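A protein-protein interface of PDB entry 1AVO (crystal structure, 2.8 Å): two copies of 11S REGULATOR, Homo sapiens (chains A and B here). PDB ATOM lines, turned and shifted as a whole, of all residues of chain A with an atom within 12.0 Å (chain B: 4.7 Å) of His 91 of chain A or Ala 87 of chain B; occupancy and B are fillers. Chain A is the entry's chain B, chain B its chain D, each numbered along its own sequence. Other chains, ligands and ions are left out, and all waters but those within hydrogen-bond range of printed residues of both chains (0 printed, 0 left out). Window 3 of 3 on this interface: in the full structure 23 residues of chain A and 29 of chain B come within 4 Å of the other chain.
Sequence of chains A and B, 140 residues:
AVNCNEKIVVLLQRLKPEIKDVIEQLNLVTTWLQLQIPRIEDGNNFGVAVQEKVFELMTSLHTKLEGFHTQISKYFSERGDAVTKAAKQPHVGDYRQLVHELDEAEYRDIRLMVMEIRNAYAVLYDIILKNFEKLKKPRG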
ATOM      1  N   ALA A  82       0.278  26.636 -11.904  1.00  0.00           N
ATOM      2  CA  ALA A  82      -0.388  27.460 -12.894  1.00  0.00           C
ATOM      3  C   ALA A  82       0.036  27.070 -14.300  1.00  0.00           C
ATOM      4  O   ALA A  82      -0.806  26.906 -15.159  1.00  0.00           O
ATOM      5  CB  ALA A  82      -0.078  28.905 -12.669  1.00  0.00           C
ATOM      6  N   VAL A  83       1.338  26.899 -14.517  1.00  0.00           N
ATOM      7  CA  VAL A  83       1.868  26.540 -15.817  1.00  0.00           C
ATOM      8  C   VAL A  83       1.265  25.244 -16.266  1.00  0.00           C
ATOM      9  O   VAL A  83       0.895  25.101 -17.413  1.00  0.00           O
ATOM     10  CB  VAL A  83       3.330  26.371 -15.744  1.00  0.00           C
ATOM     11  CG1 VAL A  83       3.830  25.948 -17.039  1.00  0.00           C
ATOM     12  CG2 VAL A  83       3.941  27.671 -15.412  1.00  0.00           C
ATOM     13  N   THR A  84       1.187  24.290 -15.354  1.00  0.00           N
ATOM     14  CA  THR A  84       0.586  22.990 -15.629  1.00  0.00           C
ATOM     15  C   THR A  84      -0.857  23.121 -16.100  1.00  0.00           C
ATOM     16  O   THR A  84      -1.199  22.556 -17.119  1.00  0.00           O
ATOM     17  CB  THR A  84       0.671  22.087 -14.386  1.00  0.00           C
ATOM     18  OG1 THR A  84       2.031  21.692 -14.205  1.00  0.00           O
ATOM     19  CG2 THR A  84      -0.157  20.873 -14.525  1.00  0.00           C
ATOM     20  N   LYS A  85      -1.708  23.837 -15.363  1.00  0.00           N
ATOM     21  CA  LYS A  85      -3.098  24.028 -15.783  1.00  0.00           C
ATOM     22  C   LYS A  85      -3.144  24.790 -17.092  1.00  0.00           C
ATOM     23  O   LYS A  85      -3.966  24.517 -17.931  1.00  0.00           O
ATOM     24  CB  LYS A  85      -3.875  24.852 -14.782  1.00  0.00           C
ATOM     25  CG  LYS A  85      -4.105  24.220 -13.461  1.00  0.00           C
ATOM     26  CD  LYS A  85      -5.085  25.082 -12.688  1.00  0.00           C
ATOM     27  CE  LYS A  85      -4.862  25.066 -11.159  1.00  0.00           C
ATOM     28  NZ  LYS A  85      -5.194  26.392 -10.469  1.00  0.00           N
ATOM     29  N   ALA A  86      -2.317  25.821 -17.224  1.00  0.00           N
ATOM     30  CA  ALA A  86      -2.272  26.626 -18.441  1.00  0.00           C
ATOM     31  C   ALA A  86      -2.086  25.674 -19.586  1.00  0.00           C
ATOM     32  O   ALA A  86      -2.818  25.733 -20.551  1.00  0.00           O
ATOM     33  CB  ALA A  86      -1.098  27.586 -18.394  1.00  0.00           C
ATOM     34  N   ALA A  87      -1.122  24.776 -19.424  1.00  0.00           N
ATOM     35  CA  ALA A  87      -0.775  23.760 -20.400  1.00  0.00           C
ATOM     36  C   ALA A  87      -1.906  22.778 -20.650  1.00  0.00           C
ATOM     37  O   ALA A  87      -2.223  22.501 -21.792  1.00  0.00           O
ATOM     38  CB  ALA A  87       0.414  23.022 -19.937  1.00  0.00           C
ATOM     39  N   LYS A  88      -2.476  22.204 -19.601  1.00  0.00           N
ATOM     40  CA  LYS A  88      -3.589  21.275 -19.755  1.00  0.00           C
ATOM     41  C   LYS A  88      -4.864  21.921 -20.277  1.00  0.00           C
ATOM     42  O   LYS A  88      -5.725  21.233 -20.773  1.00  0.00           O
ATOM     43  CB  LYS A  88      -3.940  20.640 -18.437  1.00  0.00           C
ATOM     44  CG  LYS A  88      -2.909  19.714 -17.886  1.00  0.00           C
ATOM     45  CD  LYS A  88      -3.444  19.128 -16.603  1.00  0.00           C
ATOM     46  CE  LYS A  88      -2.529  18.071 -16.005  1.00  0.00           C
ATOM     47  NZ  LYS A  88      -3.065  17.656 -14.645  1.00  0.00           N
ATOM     48  N   GLN A  89      -5.016  23.231 -20.128  1.00  0.00           N
ATOM     49  CA  GLN A  89      -6.210  23.907 -20.581  1.00  0.00           C
ATOM     50  C   GLN A  89      -5.736  25.098 -21.373  1.00  0.00           C
ATOM     51  O   GLN A  89      -5.900  26.238 -20.941  1.00  0.00           O
ATOM     52  CB  GLN A  89      -7.009  24.391 -19.384  1.00  0.00           C
ATOM     53  CG  GLN A  89      -7.129  23.389 -18.253  1.00  0.00           C
ATOM     54  CD  GLN A  89      -8.008  22.200 -18.595  1.00  0.00           C
ATOM     55  OE1 GLN A  89      -8.756  22.230 -19.572  1.00  0.00           O
ATOM     56  NE2 GLN A  89      -7.936  21.150 -17.776  1.00  0.00           N
ATOM     57  N   PRO A  90      -5.104  24.856 -22.542  1.00  0.00           N
ATOM     58  CA  PRO A  90      -4.588  25.928 -23.407  1.00  0.00           C
ATOM     59  C   PRO A  90      -5.664  26.880 -23.933  1.00  0.00           C
ATOM     60  O   PRO A  90      -5.368  27.973 -24.443  1.00  0.00           O
ATOM     61  CB  PRO A  90      -3.872  25.164 -24.515  1.00  0.00           C
ATOM     62  CG  PRO A  90      -4.615  23.913 -24.590  1.00  0.00           C
ATOM     63  CD  PRO A  90      -4.855  23.543 -23.156  1.00  0.00           C
ATOM     64  N   HIS A  91      -6.916  26.488 -23.778  1.00  0.00           N
ATOM     65  CA  HIS A  91      -7.993  27.345 -24.217  1.00  0.00           C
ATOM     66  C   HIS A  91      -8.323  28.402 -23.161  1.00  0.00           C
ATOM     67  O   HIS A  91      -8.986  29.405 -23.462  1.00  0.00           O
ATOM     68  CB  HIS A  91      -9.248  26.502 -24.533  1.00  0.00           C
ATOM     69  CG  HIS A  91      -9.635  25.526 -23.442  1.00  0.00           C
ATOM     70  ND1 HIS A  91     -10.826  25.629 -22.739  1.00  0.00           N
ATOM     71  CD2 HIS A  91      -9.013  24.424 -22.977  1.00  0.00           C
ATOM     72  CE1 HIS A  91     -10.913  24.624 -21.892  1.00  0.00           C
ATOM     73  NE2 HIS A  91      -9.834  23.872 -22.004  1.00  0.00           N
ATOM     74  N   VAL A  92      -7.910  28.146 -21.916  1.00  0.00           N
ATOM     75  CA  VAL A  92      -8.208  29.049 -20.820  1.00  0.00           C
ATOM     76  C   VAL A  92      -7.066  30.009 -20.717  1.00  0.00           C
ATOM     77  O   VAL A  92      -5.962  29.618 -20.356  1.00  0.00           O
ATOM     78  CB  VAL A  92      -8.395  28.315 -19.533  1.00  0.00           C
ATOM     79  CG1 VAL A  92      -8.985  29.226 -18.530  1.00  0.00           C
ATOM     80  CG2 VAL A  92      -9.295  27.122 -19.753  1.00  0.00           C
ATOM     81  N   GLY A  93      -7.338  31.254 -21.104  1.00  0.00           N
ATOM     82  CA  GLY A  93      -6.324  32.266 -21.113  1.00  0.00           C
ATOM     83  C   GLY A  93      -5.997  32.834 -19.766  1.00  0.00           C
ATOM     84  O   GLY A  93      -4.943  33.462 -19.599  1.00  0.00           O
ATOM     85  N   ASP A  94      -6.896  32.642 -18.805  1.00  0.00           N
ATOM     86  CA  ASP A  94      -6.685  33.157 -17.457  1.00  0.00           C
ATOM     87  C   ASP A  94      -5.522  32.474 -16.776  1.00  0.00           C
ATOM     88  O   ASP A  94      -4.852  33.077 -15.938  1.00  0.00           O
ATOM     89  CB  ASP A  94      -7.953  33.050 -16.639  1.00  0.00           C
ATOM     90  CG  ASP A  94      -9.101  33.775 -17.300  1.00  0.00           C
ATOM     91  OD1 ASP A  94      -9.805  33.145 -18.142  1.00  0.00           O
ATOM     92  OD2 ASP A  94      -9.269  34.983 -17.040  1.00  0.00           O
ATOM     93  N   TYR A  95      -5.225  31.246 -17.193  1.00  0.00           N
ATOM     94  CA  TYR A  95      -4.112  30.525 -16.616  1.00  0.00           C
ATOM     95  C   TYR A  95      -2.787  31.085 -17.117  1.00  0.00           C
ATOM     96  O   TYR A  95      -1.787  31.083 -16.393  1.00  0.00           O
ATOM     97  CB  TYR A  95      -4.215  29.037 -16.917  1.00  0.00           C
ATOM     98  CG  TYR A  95      -5.333  28.314 -16.173  1.00  0.00           C
ATOM     99  CD1 TYR A  95      -5.698  28.687 -14.878  1.00  0.00           C
ATOM    100  CD2 TYR A  95      -6.025  27.268 -16.768  1.00  0.00           C
ATOM    101  CE1 TYR A  95      -6.718  28.043 -14.219  1.00  0.00           C
ATOM    102  CE2 TYR A  95      -7.039  26.629 -16.111  1.00  0.00           C
ATOM    103  CZ  TYR A  95      -7.377  27.024 -14.848  1.00  0.00           C
ATOM    104  OH  TYR A  95      -8.397  26.391 -14.215  1.00  0.00           O
ATOM    105  N   ARG A  96      -2.754  31.600 -18.334  1.00  0.00           N
ATOM    106  CA  ARG A  96      -1.496  32.146 -18.792  1.00  0.00           C
ATOM    107  C   ARG A  96      -1.320  33.466 -18.115  1.00  0.00           C
ATOM    108  O   ARG A  96      -0.199  33.818 -17.734  1.00  0.00           O
ATOM    109  CB  ARG A  96      -1.450  32.333 -20.285  1.00  0.00           C
ATOM    110  CG  ARG A  96      -1.351  31.048 -21.045  1.00  0.00           C
ATOM    111  CD  ARG A  96      -2.030  31.240 -22.378  1.00  0.00           C
ATOM    112  NE  ARG A  96      -2.469  30.001 -22.996  1.00  0.00           N
ATOM    113  CZ  ARG A  96      -1.774  29.383 -23.947  1.00  0.00           C
ATOM    114  NH1 ARG A  96      -0.607  29.887 -24.383  1.00  0.00           N
ATOM    115  NH2 ARG A  96      -2.244  28.259 -24.464  1.00  0.00           N
ATOM    116  N   GLN A  97      -2.430  34.182 -17.928  1.00  0.00           N
ATOM    117  CA  GLN A  97      -2.326  35.467 -17.264  1.00  0.00           C
ATOM    118  C   GLN A  97      -1.927  35.275 -15.801  1.00  0.00           C
ATOM    119  O   GLN A  97      -1.130  36.034 -15.260  1.00  0.00           O
ATOM    120  CB  GLN A  97      -3.619  36.239 -17.352  1.00  0.00           C
ATOM    121  CG  GLN A  97      -3.572  37.406 -18.292  1.00  0.00           C
ATOM    122  CD  GLN A  97      -2.675  38.533 -17.797  1.00  0.00           C
ATOM    123  OE1 GLN A  97      -1.607  38.785 -18.377  1.00  0.00           O
ATOM    124  NE2 GLN A  97      -3.116  39.241 -16.750  1.00  0.00           N
ATOM    125  N   LEU A  98      -2.473  34.241 -15.172  1.00  0.00           N
ATOM    126  CA  LEU A  98      -2.174  33.951 -13.782  1.00  0.00           C
ATOM    127  C   LEU A  98      -0.688  33.763 -13.671  1.00  0.00           C
ATOM    128  O   LEU A  98      -0.051  34.395 -12.844  1.00  0.00           O
ATOM    129  CB  LEU A  98      -2.854  32.679 -13.340  1.00  0.00           C
ATOM    130  CG  LEU A  98      -2.583  32.340 -11.889  1.00  0.00           C
ATOM    131  CD1 LEU A  98      -2.844  33.551 -10.993  1.00  0.00           C
ATOM    132  CD2 LEU A  98      -3.487  31.206 -11.509  1.00  0.00           C
ATOM    133  N   ALA B   1      -9.972  29.958 -28.324  1.00  0.00           N
ATOM    134  CA  ALA B   1      -9.561  30.117 -26.894  1.00  0.00           C
ATOM    135  C   ALA B   1     -10.444  31.093 -26.119  1.00  0.00           C
ATOM    136  O   ALA B   1     -10.971  32.028 -26.711  1.00  0.00           O
ATOM    137  CB  ALA B   1      -8.099  30.590 -26.814  1.00  0.00           C
ATOM    138  N   VAL B   2     -10.610  30.893 -24.808  1.00  0.00           N
ATOM    139  CA  VAL B   2     -11.401  31.817 -24.012  1.00  0.00           C
ATOM    140  C   VAL B   2     -10.449  32.768 -23.320  1.00  0.00           C
ATOM    141  O   VAL B   2      -9.629  32.371 -22.500  1.00  0.00           O
ATOM    142  CB  VAL B   2     -12.210  31.134 -22.981  1.00  0.00           C
ATOM    143  CG1 VAL B   2     -13.156  32.121 -22.352  1.00  0.00           C
ATOM    144  CG2 VAL B   2     -12.961  30.033 -23.598  1.00  0.00           C
ATOM    145  N   VAL B  83     -14.175  28.994 -16.204  1.00  0.00           N
ATOM    146  CA  VAL B  83     -14.202  28.740 -17.655  1.00  0.00           C
ATOM    147  C   VAL B  83     -13.996  27.254 -17.917  1.00  0.00           C
ATOM    148  O   VAL B  83     -14.736  26.632 -18.681  1.00  0.00           O
ATOM    149  CB  VAL B  83     -13.055  29.444 -18.365  1.00  0.00           C
ATOM    150  CG1 VAL B  83     -13.010  29.008 -19.779  1.00  0.00           C
ATOM    151  CG2 VAL B  83     -13.233  30.908 -18.323  1.00  0.00           C
ATOM    152  N   THR B  84     -12.947  26.721 -17.297  1.00  0.00           N
ATOM    153  CA  THR B  84     -12.635  25.322 -17.420  1.00  0.00           C
ATOM    154  C   THR B  84     -13.841  24.424 -17.142  1.00  0.00           C
ATOM    155  O   THR B  84     -14.150  23.596 -17.986  1.00  0.00           O
ATOM    156  CB  THR B  84     -11.483  24.949 -16.518  1.00  0.00           C
ATOM    157  OG1 THR B  84     -10.286  25.559 -17.007  1.00  0.00           O
ATOM    158  CG2 THR B  84     -11.290  23.488 -16.510  1.00  0.00           C
ATOM    159  N   LYS B  85     -14.533  24.597 -16.010  1.00  0.00           N
ATOM    160  CA  LYS B  85     -15.716  23.781 -15.683  1.00  0.00           C
ATOM    161  C   LYS B  85     -16.814  24.065 -16.657  1.00  0.00           C
ATOM    162  O   LYS B  85     -17.550  23.156 -17.031  1.00  0.00           O
ATOM    163  CB  LYS B  85     -16.285  24.088 -14.312  1.00  0.00           C
ATOM    164  CG  LYS B  85     -15.457  23.639 -13.150  1.00  0.00           C
ATOM    165  CD  LYS B  85     -16.226  23.861 -11.867  1.00  0.00           C
ATOM    166  CE  LYS B  85     -15.345  24.252 -10.678  1.00  0.00           C
ATOM    167  NZ  LYS B  85     -16.095  25.174  -9.736  1.00  0.00           N
ATOM    168  N   ALA B  86     -16.968  25.343 -16.996  1.00  0.00           N
ATOM    169  CA  ALA B  86     -18.000  25.764 -17.928  1.00  0.00           C
ATOM    170  C   ALA B  86     -17.808  24.936 -19.186  1.00  0.00           C
ATOM    171  O   ALA B  86     -18.741  24.303 -19.672  1.00  0.00           O
ATOM    172  CB  ALA B  86     -17.840  27.229 -18.236  1.00  0.00           C
ATOM    173  N   ALA B  87     -16.559  24.899 -19.648  1.00  0.00           N
ATOM    174  CA  ALA B  87     -16.141  24.158 -20.839  1.00  0.00           C
ATOM    175  C   ALA B  87     -16.371  22.676 -20.686  1.00  0.00           C
ATOM    176  O   ALA B  87     -16.939  22.062 -21.570  1.00  0.00           O
ATOM    177  CB  ALA B  87     -14.690  24.390 -21.118  1.00  0.00           C
ATOM    178  N   LYS B  88     -15.892  22.085 -19.598  1.00  0.00           N
ATOM    179  CA  LYS B  88     -16.087  20.652 -19.363  1.00  0.00           C
ATOM    180  C   LYS B  88     -17.528  20.246 -19.137  1.00  0.00           C
ATOM    181  O   LYS B  88     -17.865  19.088 -19.287  1.00  0.00           O
ATOM    182  CB  LYS B  88     -15.315  20.175 -18.153  1.00  0.00           C
ATOM    183  CG  LYS B  88     -13.835  20.188 -18.310  1.00  0.00           C
ATOM    184  CD  LYS B  88     -13.193  19.643 -17.045  1.00  0.00           C
ATOM    185  CE  LYS B  88     -11.655  19.556 -17.135  1.00  0.00           C
ATOM    186  NZ  LYS B  88     -11.091  19.185 -15.794  1.00  0.00           N
ATOM    187  N   GLN B  89     -18.366  21.172 -18.697  1.00  0.00           N
ATOM    188  CA  GLN B  89     -19.749  20.848 -18.443  1.00  0.00           C
ATOM    189  C   GLN B  89     -20.569  21.893 -19.153  1.00  0.00           C
ATOM    190  O   GLN B  89     -21.215  22.719 -18.521  1.00  0.00           O
ATOM    191  CB  GLN B  89     -20.002  20.927 -16.959  1.00  0.00           C
ATOM    192  CG  GLN B  89     -18.909  20.322 -16.126  1.00  0.00           C
ATOM    193  CD  GLN B  89     -18.867  18.815 -16.224  1.00  0.00           C
ATOM    194  OE1 GLN B  89     -19.796  18.193 -16.727  1.00  0.00           O
ATOM    195  NE2 GLN B  89     -17.790  18.217 -15.729  1.00  0.00           N
ATOM    196  N   PRO B  90     -20.554  21.875 -20.496  1.00  0.00           N
ATOM    197  CA  PRO B  90     -21.307  22.847 -21.307  1.00  0.00           C
ATOM    198  C   PRO B  90     -22.806  22.789 -21.129  1.00  0.00           C
ATOM    199  O   PRO B  90     -23.523  23.686 -21.569  1.00  0.00           O
ATOM    200  CB  PRO B  90     -20.892  22.505 -22.739  1.00  0.00           C
ATOM    201  CG  PRO B  90     -20.594  21.055 -22.656  1.00  0.00           C
ATOM    202  CD  PRO B  90     -19.850  20.913 -21.356  1.00  0.00           C
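The backbone NH (N) of Val 2 of chain B is in hydrogen-bond range of the backbone carbonyl oxygen (O) of His 91 of chain A, 2.6 Å away.
N of Gly 93 of chain A is in hydrogen-bond range of O of Val 2 of chain B, 2.9 Å away.
OG1 of Thr 84 of chain B sits at hydrogen-bond distance from OH of Tyr 95 of chain A.
8 positions are printed for both chains.
Of the 7 pairs that touch across the chains among the printed residues, none has its exchanged pair printed and touching as well.
His 91 of chain A touches Ala 1 of chain B.
His 91 of chain A touches Ala 87 of chain B.
C of Val 92 of chain A touches O of Val 2 of chain B, at 3.9 Å.
CG2 of Val 92 of chain A touches OG1 of Thr 84 of chain B (3.3 Å).
Printed residues of chain A that touch a printed residue of chain B: His 91, Val 92, Gly 93 and Tyr 95.
Hydrophobic or aromatic side chains of chain A that line the printed part of chain B: His 91, Val 92 and Tyr 95.
Along chain A the printed residues that touch a printed residue of chain B span positions 91 to 95.
Of the 10 printed residues of chain B, 4 touch a printed residue of chain A.
Hydrophobic or aromatic side chains of chain B that line the printed part of chain A: Ala 1, Val 2 and Ala 87.
The side-chain amide oxygen (OE1) of Gln 89 of chain A is in hydrogen-bond range of a ring nitrogen (NE2) of His 91 of chain A (3.1 Å).
Gln 89 of chain A touches none of the printed residues of chain B.
His 91 of chain A touches just these residues of chain B: Ala 1 (3.5 Å), Val 2 (2.6 Å) and Ala 87 (3.9 Å).
Of the printed residues of chain B, Val 92 of chain A touches Val 2 and Thr 84.
Printed residues of chain B within 4 Å of Gly 93 of chain A: Val 2.
Of the printed residues of chain B, Tyr 95 of chain A touches Thr 84.
Arg 96 of chain A touches none of the printed residues of chain B.
Of chain A, only His 91 comes within 4 Å of Ala 1 of chain B.
Val 2 of chain B touches just these residues of chain A: His 91, Val 92 and Gly 93.
Val 83 of chain B touches none of the printed residues of chain A.
Thr 84 of chain B touches just these residues of chain A: Val 92 and Tyr 95.
No residue of chain A comes within 4 Å of Ala 86 of chain B.
Ala 87 of chain B touches just one residue of chain A: His 91 (3.9 Å).
No residue of chain A comes within 4 Å of Lys 88 of chain B.
Pro 90 of chain B touches none of the printed residues of chain A.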
